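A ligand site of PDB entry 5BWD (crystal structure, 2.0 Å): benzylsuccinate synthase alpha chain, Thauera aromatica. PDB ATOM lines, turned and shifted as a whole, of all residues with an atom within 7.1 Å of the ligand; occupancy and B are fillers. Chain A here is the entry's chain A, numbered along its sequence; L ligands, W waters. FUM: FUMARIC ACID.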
ATOM      1  N   GLU A 188     -10.864 -33.572  12.530  1.00  0.00           N
ATOM      2  CA  GLU A 188     -12.318 -33.530  12.658  1.00  0.00           C
ATOM      3  C   GLU A 188     -12.877 -32.887  11.395  1.00  0.00           C
ATOM      4  O   GLU A 188     -12.286 -31.964  10.846  1.00  0.00           O
ATOM      5  CB  GLU A 188     -12.752 -32.751  13.899  1.00  0.00           C
ATOM      6  CG  GLU A 188     -14.265 -32.646  14.055  1.00  0.00           C
ATOM      7  CD  GLU A 188     -14.682 -31.908  15.307  1.00  0.00           C
ATOM      8  OE1 GLU A 188     -15.890 -31.602  15.446  1.00  0.00           O
ATOM      9  OE2 GLU A 188     -13.812 -31.626  16.159  1.00  0.00           O
ATOM     10  N   SER A 191     -16.967 -27.890  10.589  1.00  0.00           N
ATOM     11  CA  SER A 191     -18.329 -27.669  11.068  1.00  0.00           C
ATOM     12  C   SER A 191     -19.339 -27.415   9.952  1.00  0.00           C
ATOM     13  O   SER A 191     -20.520 -27.709  10.117  1.00  0.00           O
ATOM     14  CB  SER A 191     -18.359 -26.504  12.062  1.00  0.00           C
ATOM     15  OG  SER A 191     -17.794 -26.886  13.297  1.00  0.00           O
ATOM     16  N   TYR A 196     -22.561 -28.850  13.101  1.00  0.00           N
ATOM     17  CA  TYR A 196     -22.237 -28.684  14.516  1.00  0.00           C
ATOM     18  C   TYR A 196     -21.765 -27.255  14.772  1.00  0.00           C
ATOM     19  O   TYR A 196     -21.213 -26.612  13.874  1.00  0.00           O
ATOM     20  CB  TYR A 196     -21.165 -29.691  14.955  1.00  0.00           C
ATOM     21  CG  TYR A 196     -21.071 -29.888  16.448  1.00  0.00           C
ATOM     22  CD1 TYR A 196     -22.057 -30.576  17.141  1.00  0.00           C
ATOM     23  CD2 TYR A 196     -19.983 -29.398  17.165  1.00  0.00           C
ATOM     24  CE1 TYR A 196     -21.966 -30.760  18.508  1.00  0.00           C
ATOM     25  CE2 TYR A 196     -19.886 -29.576  18.528  1.00  0.00           C
ATOM     26  CZ  TYR A 196     -20.880 -30.253  19.201  1.00  0.00           C
ATOM     27  OH  TYR A 196     -20.789 -30.437  20.568  1.00  0.00           O
ATOM     28  N   ASN A 197     -22.002 -26.752  15.976  1.00  0.00           N
ATOM     29  CA  ASN A 197     -21.816 -25.341  16.264  1.00  0.00           C
ATOM     30  C   ASN A 197     -21.818 -25.095  17.771  1.00  0.00           C
ATOM     31  O   ASN A 197     -22.178 -25.972  18.548  1.00  0.00           O
ATOM     32  CB  ASN A 197     -22.917 -24.514  15.589  1.00  0.00           C
ATOM     33  CG  ASN A 197     -22.650 -23.016  15.618  1.00  0.00           C
ATOM     34  OD1 ASN A 197     -21.506 -22.577  15.491  1.00  0.00           O
ATOM     35  ND2 ASN A 197     -23.712 -22.232  15.791  1.00  0.00           N
ATOM     36  N   SER A 198     -21.409 -23.896  18.178  1.00  0.00           N
ATOM     37  CA  SER A 198     -21.511 -23.468  19.566  1.00  0.00           C
ATOM     38  C   SER A 198     -21.763 -21.963  19.592  1.00  0.00           C
ATOM     39  O   SER A 198     -21.585 -21.285  18.579  1.00  0.00           O
ATOM     40  CB  SER A 198     -20.240 -23.812  20.342  1.00  0.00           C
ATOM     41  OG  SER A 198     -19.107 -23.156  19.797  1.00  0.00           O
ATOM     42  N   LEU A 390     -24.269 -31.617  24.670  1.00  0.00           N
ATOM     43  CA  LEU A 390     -23.366 -31.052  25.658  1.00  0.00           C
ATOM     44  C   LEU A 390     -23.913 -29.729  26.179  1.00  0.00           C
ATOM     45  O   LEU A 390     -24.008 -28.768  25.421  1.00  0.00           O
ATOM     46  CB  LEU A 390     -21.965 -30.838  25.082  1.00  0.00           C
ATOM     47  CG  LEU A 390     -21.186 -32.057  24.596  1.00  0.00           C
ATOM     48  CD1 LEU A 390     -19.921 -31.618  23.866  1.00  0.00           C
ATOM     49  CD2 LEU A 390     -20.842 -32.974  25.765  1.00  0.00           C
ATOM     50  N   ILE A 392     -22.954 -27.110  29.068  1.00  0.00           N
ATOM     51  CA  ILE A 392     -22.013 -26.740  30.129  1.00  0.00           C
ATOM     52  C   ILE A 392     -22.177 -25.291  30.550  1.00  0.00           C
ATOM     53  O   ILE A 392     -21.896 -24.375  29.783  1.00  0.00           O
ATOM     54  CB  ILE A 392     -20.567 -27.009  29.707  1.00  0.00           C
ATOM     55  CG1 ILE A 392     -20.369 -28.471  29.293  1.00  0.00           C
ATOM     56  CG2 ILE A 392     -19.619 -26.648  30.834  1.00  0.00           C
ATOM     57  CD1 ILE A 392     -20.439 -28.700  27.797  1.00  0.00           C
ATOM     58  N   ASN A 489     -16.822 -21.266  30.085  1.00  0.00           N
ATOM     59  CA  ASN A 489     -16.425 -22.251  29.092  1.00  0.00           C
ATOM     60  C   ASN A 489     -17.440 -22.231  27.953  1.00  0.00           C
ATOM     61  O   ASN A 489     -18.648 -22.182  28.182  1.00  0.00           O
ATOM     62  CB  ASN A 489     -16.321 -23.646  29.719  1.00  0.00           C
ATOM     63  CG  ASN A 489     -14.966 -23.892  30.368  1.00  0.00           C
ATOM     64  OD1 ASN A 489     -14.204 -22.955  30.601  1.00  0.00           O
ATOM     65  ND2 ASN A 489     -14.646 -25.159  30.628  1.00  0.00           N
ATOM     66  N   VAL A 490     -16.942 -22.240  26.723  1.00  0.00           N
ATOM     67  CA  VAL A 490     -17.811 -22.223  25.545  1.00  0.00           C
ATOM     68  C   VAL A 490     -18.545 -23.551  25.458  1.00  0.00           C
ATOM     69  O   VAL A 490     -19.780 -23.593  25.469  1.00  0.00           O
ATOM     70  CB  VAL A 490     -17.003 -21.952  24.259  1.00  0.00           C
ATOM     71  CG1 VAL A 490     -17.924 -21.956  23.043  1.00  0.00           C
ATOM     72  CG2 VAL A 490     -16.263 -20.626  24.377  1.00  0.00           C
ATOM     73  N   LEU A 491     -17.792 -24.636  25.380  1.00  0.00           N
ATOM     74  CA  LEU A 491     -18.353 -25.960  25.557  1.00  0.00           C
ATOM     75  C   LEU A 491     -17.686 -26.608  26.766  1.00  0.00           C
ATOM     76  O   LEU A 491     -17.880 -26.157  27.890  1.00  0.00           O
ATOM     77  CB  LEU A 491     -18.162 -26.817  24.303  1.00  0.00           C
ATOM     78  CG  LEU A 491     -18.937 -26.354  23.056  1.00  0.00           C
ATOM     79  CD1 LEU A 491     -18.766 -27.329  21.901  1.00  0.00           C
ATOM     80  CD2 LEU A 491     -20.397 -26.181  23.389  1.00  0.00           C
ATOM     81  N   CYS A 492     -16.898 -27.643  26.537  1.00  0.00           N
ATOM     82  CA  CYS A 492     -16.294 -28.397  27.638  1.00  0.00           C
ATOM     83  C   CYS A 492     -15.103 -27.686  28.276  1.00  0.00           C
ATOM     84  O   CYS A 492     -15.015 -27.602  29.495  1.00  0.00           O
ATOM     85  CB  CYS A 492     -15.859 -29.781  27.161  1.00  0.00           C
ATOM     86  SG  CYS A 492     -17.212 -30.884  26.685  1.00  0.00           S
ATOM     87  N   MET A 493     -14.185 -27.180  27.447  1.00  0.00           N
ATOM     88  CA  MET A 493     -12.855 -26.836  27.945  1.00  0.00           C
ATOM     89  C   MET A 493     -12.346 -25.433  27.644  1.00  0.00           C
ATOM     90  O   MET A 493     -11.396 -24.970  28.277  1.00  0.00           O
ATOM     91  CB  MET A 493     -11.857 -27.848  27.393  1.00  0.00           C
ATOM     92  CG  MET A 493     -11.846 -29.172  28.122  1.00  0.00           C
ATOM     93  SD  MET A 493     -11.324 -28.976  29.829  1.00  0.00           S
ATOM     94  CE  MET A 493      -9.822 -28.027  29.614  1.00  0.00           C
ATOM     95  N   SER A 494     -12.962 -24.737  26.695  1.00  0.00           N
ATOM     96  CA  SER A 494     -12.387 -23.476  26.217  1.00  0.00           C
ATOM     97  C   SER A 494     -13.043 -22.232  26.807  1.00  0.00           C
ATOM     98  O   SER A 494     -14.246 -22.051  26.705  1.00  0.00           O
ATOM     99  CB  SER A 494     -12.467 -23.417  24.686  1.00  0.00           C
ATOM    100  OG  SER A 494     -11.847 -22.246  24.191  1.00  0.00           O
ATOM    101  N   PRO A 495     -12.226 -21.366  27.434  1.00  0.00           N
ATOM    102  CA  PRO A 495     -12.708 -20.102  27.990  1.00  0.00           C
ATOM    103  C   PRO A 495     -13.168 -19.108  26.921  1.00  0.00           C
ATOM    104  O   PRO A 495     -12.634 -19.078  25.824  1.00  0.00           O
ATOM    105  CB  PRO A 495     -11.490 -19.552  28.733  1.00  0.00           C
ATOM    106  CG  PRO A 495     -10.623 -20.731  28.966  1.00  0.00           C
ATOM    107  CD  PRO A 495     -10.817 -21.619  27.785  1.00  0.00           C
ATOM    108  N   GLN A 504     -18.335 -14.956  22.039  1.00  0.00           N
ATOM    109  CA  GLN A 504     -18.126 -15.773  20.849  1.00  0.00           C
ATOM    110  C   GLN A 504     -19.465 -16.212  20.270  1.00  0.00           C
ATOM    111  O   GLN A 504     -20.342 -16.687  20.994  1.00  0.00           O
ATOM    112  CB  GLN A 504     -17.262 -16.992  21.180  1.00  0.00           C
ATOM    113  CG  GLN A 504     -17.134 -17.992  20.040  1.00  0.00           C
ATOM    114  CD  GLN A 504     -16.074 -19.033  20.299  1.00  0.00           C
ATOM    115  OE1 GLN A 504     -15.172 -18.833  21.104  1.00  0.00           O
ATOM    116  NE2 GLN A 504     -16.187 -20.175  19.610  1.00  0.00           N
ATOM    117  N   ARG A 507     -18.838 -21.536  16.410  1.00  0.00           N
ATOM    118  CA  ARG A 507     -17.743 -22.484  16.555  1.00  0.00           C
ATOM    119  C   ARG A 507     -16.678 -22.249  15.486  1.00  0.00           C
ATOM    120  O   ARG A 507     -15.559 -22.760  15.587  1.00  0.00           O
ATOM    121  CB  ARG A 507     -18.271 -23.931  16.466  1.00  0.00           C
ATOM    122  CG  ARG A 507     -17.261 -24.991  16.855  1.00  0.00           C
ATOM    123  CD  ARG A 507     -17.917 -26.359  16.940  1.00  0.00           C
ATOM    124  NE  ARG A 507     -17.032 -27.367  17.517  1.00  0.00           N
ATOM    125  CZ  ARG A 507     -16.610 -28.451  16.879  1.00  0.00           C
ATOM    126  NH1 ARG A 507     -16.988 -28.672  15.625  1.00  0.00           N
ATOM    127  NH2 ARG A 507     -15.813 -29.314  17.486  1.00  0.00           N
ATOM    128  N   GLY A 510     -13.702 -20.618  17.164  1.00  0.00           N
ATOM    129  CA  GLY A 510     -12.863 -21.563  17.878  1.00  0.00           C
ATOM    130  C   GLY A 510     -13.575 -22.859  18.192  1.00  0.00           C
ATOM    131  O   GLY A 510     -14.771 -22.869  18.494  1.00  0.00           O
ATOM    132  N   GLY A 511     -12.838 -23.962  18.136  1.00  0.00           N
ATOM    133  CA  GLY A 511     -13.418 -25.283  18.288  1.00  0.00           C
ATOM    134  C   GLY A 511     -13.051 -26.158  17.109  1.00  0.00           C
ATOM    135  O   GLY A 511     -12.582 -25.660  16.085  1.00  0.00           O
ATOM    136  N   GLY A 512     -13.277 -27.461  17.239  1.00  0.00           N
ATOM    137  CA  GLY A 512     -12.854 -28.406  16.226  1.00  0.00           C
ATOM    138  C   GLY A 512     -11.635 -29.157  16.704  1.00  0.00           C
ATOM    139  O   GLY A 512     -10.889 -28.660  17.545  1.00  0.00           O
ATOM    140  N   SER A 513     -11.416 -30.354  16.176  1.00  0.00           N
ATOM    141  CA  SER A 513     -10.371 -31.231  16.696  1.00  0.00           C
ATOM    142  C   SER A 513      -9.329 -31.641  15.674  1.00  0.00           C
ATOM    143  O   SER A 513      -9.555 -31.591  14.465  1.00  0.00           O
ATOM    144  CB  SER A 513     -11.004 -32.479  17.313  1.00  0.00           C
ATOM    145  OG  SER A 513     -11.994 -32.140  18.265  1.00  0.00           O
ATOM    146  N   TRP A 612      -9.147 -21.240  18.630  1.00  0.00           N
ATOM    147  CA  TRP A 612      -8.547 -22.449  19.182  1.00  0.00           C
ATOM    148  C   TRP A 612      -8.940 -23.678  18.387  1.00  0.00           C
ATOM    149  O   TRP A 612      -9.912 -23.659  17.634  1.00  0.00           O
ATOM    150  CB  TRP A 612      -8.945 -22.636  20.646  1.00  0.00           C
ATOM    151  CG  TRP A 612     -10.238 -23.367  20.888  1.00  0.00           C
ATOM    152  CD1 TRP A 612     -10.409 -24.723  20.933  1.00  0.00           C
ATOM    153  CD2 TRP A 612     -11.525 -22.796  21.132  1.00  0.00           C
ATOM    154  NE1 TRP A 612     -11.727 -25.020  21.189  1.00  0.00           N
ATOM    155  CE2 TRP A 612     -12.435 -23.856  21.310  1.00  0.00           C
ATOM    156  CE3 TRP A 612     -11.996 -21.484  21.221  1.00  0.00           C
ATOM    157  CZ2 TRP A 612     -13.784 -23.640  21.569  1.00  0.00           C
ATOM    158  CZ3 TRP A 612     -13.344 -21.278  21.470  1.00  0.00           C
ATOM    159  CH2 TRP A 612     -14.217 -22.346  21.643  1.00  0.00           C
ATOM    160  N   HIS A 613      -8.175 -24.745  18.560  1.00  0.00           N
ATOM    161  CA  HIS A 613      -8.482 -26.047  17.995  1.00  0.00           C
ATOM    162  C   HIS A 613      -8.083 -27.107  19.016  1.00  0.00           C
ATOM    163  O   HIS A 613      -7.186 -26.872  19.817  1.00  0.00           O
ATOM    164  CB  HIS A 613      -7.765 -26.259  16.659  1.00  0.00           C
ATOM    165  CG  HIS A 613      -8.559 -27.050  15.668  1.00  0.00           C
ATOM    166  ND1 HIS A 613      -9.581 -26.510  14.926  1.00  0.00           N
ATOM    167  CD2 HIS A 613      -8.475 -28.352  15.294  1.00  0.00           C
ATOM    168  CE1 HIS A 613     -10.096 -27.434  14.137  1.00  0.00           C
ATOM    169  NE2 HIS A 613      -9.441 -28.558  14.341  1.00  0.00           N
ATOM    170  N   ASN A 614      -8.753 -28.252  18.989  1.00  0.00           N
ATOM    171  CA  ASN A 614      -8.543 -29.272  20.017  1.00  0.00           C
ATOM    172  C   ASN A 614      -7.608 -30.386  19.570  1.00  0.00           C
ATOM    173  O   ASN A 614      -7.985 -31.230  18.755  1.00  0.00           O
ATOM    174  CB  ASN A 614      -9.888 -29.886  20.422  1.00  0.00           C
ATOM    175  CG  ASN A 614     -10.963 -28.846  20.691  1.00  0.00           C
ATOM    176  OD1 ASN A 614     -10.683 -27.758  21.183  1.00  0.00           O
ATOM    177  ND2 ASN A 614     -12.204 -29.182  20.362  1.00  0.00           N
ATOM    178  N   THR A 704      -6.424 -26.494  22.628  1.00  0.00           N
ATOM    179  CA  THR A 704      -7.248 -26.863  23.771  1.00  0.00           C
ATOM    180  C   THR A 704      -7.368 -28.395  23.845  1.00  0.00           C
ATOM    181  O   THR A 704      -8.212 -28.986  23.183  1.00  0.00           O
ATOM    182  CB  THR A 704      -8.657 -26.245  23.716  1.00  0.00           C
ATOM    183  OG1 THR A 704      -8.549 -24.821  23.724  1.00  0.00           O
ATOM    184  CG2 THR A 704      -9.488 -26.684  24.909  1.00  0.00           C
ATOM    185  N   GLN A 706      -8.385 -31.987  24.971  1.00  0.00           N
ATOM    186  CA  GLN A 706      -9.539 -32.617  25.612  1.00  0.00           C
ATOM    187  C   GLN A 706      -9.945 -33.902  24.902  1.00  0.00           C
ATOM    188  O   GLN A 706      -9.205 -34.417  24.061  1.00  0.00           O
ATOM    189  CB  GLN A 706     -10.732 -31.643  25.635  1.00  0.00           C
ATOM    190  CG  GLN A 706     -10.996 -30.943  24.318  1.00  0.00           C
ATOM    191  CD  GLN A 706     -12.098 -29.903  24.431  1.00  0.00           C
ATOM    192  OE1 GLN A 706     -13.082 -30.107  25.137  1.00  0.00           O
ATOM    193  NE2 GLN A 706     -11.931 -28.783  23.740  1.00  0.00           N
HETATM  194  OXT FUM L   1     -16.159 -26.613  20.047  1.00  0.00           O
HETATM  195  C   FUM L   1     -15.301 -27.450  20.415  1.00  0.00           C
HETATM  196  O   FUM L   1     -14.859 -28.316  19.638  1.00  0.00           O
HETATM  197  C4  FUM L   1     -14.796 -27.406  21.807  1.00  0.00           C
HETATM  198  C5  FUM L   1     -15.188 -26.432  22.631  1.00  0.00           C
HETATM  199  C6  FUM L   1     -14.683 -26.389  24.023  1.00  0.00           C
HETATM  200  O7  FUM L   1     -13.911 -27.291  24.423  1.00  0.00           O
HETATM  201  O8  FUM L   1     -15.038 -25.445  24.766  1.00  0.00           O
HETATM  202  O   HOH W   1     -16.048 -29.718  23.952  1.00  0.00           O
HETATM  203  O   HOH W   2     -16.676 -23.872  20.266  1.00  0.00           O
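Residues that only touch the ligand: Trp 612 (3.3 Å) and Gly 511 (3.5 Å).
Hydrophobic or aromatic side chains within 4 Å of the ligand: Leu 491, Met 493 and Trp 612.
N of Arg 507 lies within hydrogen-bond range of OD1 of Asn 197 (3.0 Å).
The guanidinium group (NH1) of Arg 507 sits at hydrogen-bond distance from the side-chain hydroxyl (OG) of Ser 191 (3.0 Å).
NE2 of Gln 706 is in hydrogen-bond range of OD1 of Asn 614, at 3.0 Å.
The side-chain amide oxygen of Asn 614 is in hydrogen-bond range of the indole nitrogen of Trp 612 (2.9 Å).
OD1 of Asn 614 sits close to O of Thr 704 (3.4 Å).
O of Trp 612 lies within hydrogen-bond range of N of Gly 511 (3.0 Å).
The side-chain amide nitrogen (ND2) of Asn 489 sits at hydrogen-bond distance from the backbone carbonyl oxygen (O) of Cys 492, 2.7 Å away.
O of Gly 511 is in hydrogen-bond range of ND1 of His 613 (3.3 Å).
Water W2 lies within hydrogen-bond range of the side-chain hydroxyl of Ser 198 (2.6 Å), the backbone carbonyl oxygen of Gly 510 (2.8 Å) and an oxygen (OXT) of the ligand (2.8 Å).
Water W1 lies within hydrogen-bond range of the side-chain sulfur of Cys 492 (3.2 Å), the side-chain amide oxygen of Gln 706 (3.2 Å) and an oxygen (O7) of the ligand (3.3 Å).
The guanidinium group (NH2) of Arg 507 lies within salt-bridge range of an oxygen (O) of the ligand (2.6 Å).
The side-chain amide nitrogen (NE2) of Gln 706 sits at hydrogen-bond distance from an oxygen (O7) of the ligand, 2.6 Å away.
ND2 of Asn 614 is in hydrogen-bond range of O of the ligand (2.9 Å).
N of Ser 494 is in hydrogen-bond range of O8 of the ligand, 2.9 Å away.
The backbone NH (N) of Leu 491 lies within hydrogen-bond range of an oxygen (O8) of the ligand.
N of Gly 512 sits at hydrogen-bond distance from O of the ligand (3.0 Å).
An oxygen (O7) of the ligand lies within hydrogen-bond range of the backbone NH (N) of Met 493, 3.0 Å away.
The backbone NH (N) of Cys 492 sits at hydrogen-bond distance from an oxygen (O8) of the ligand, at 3.4 Å.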
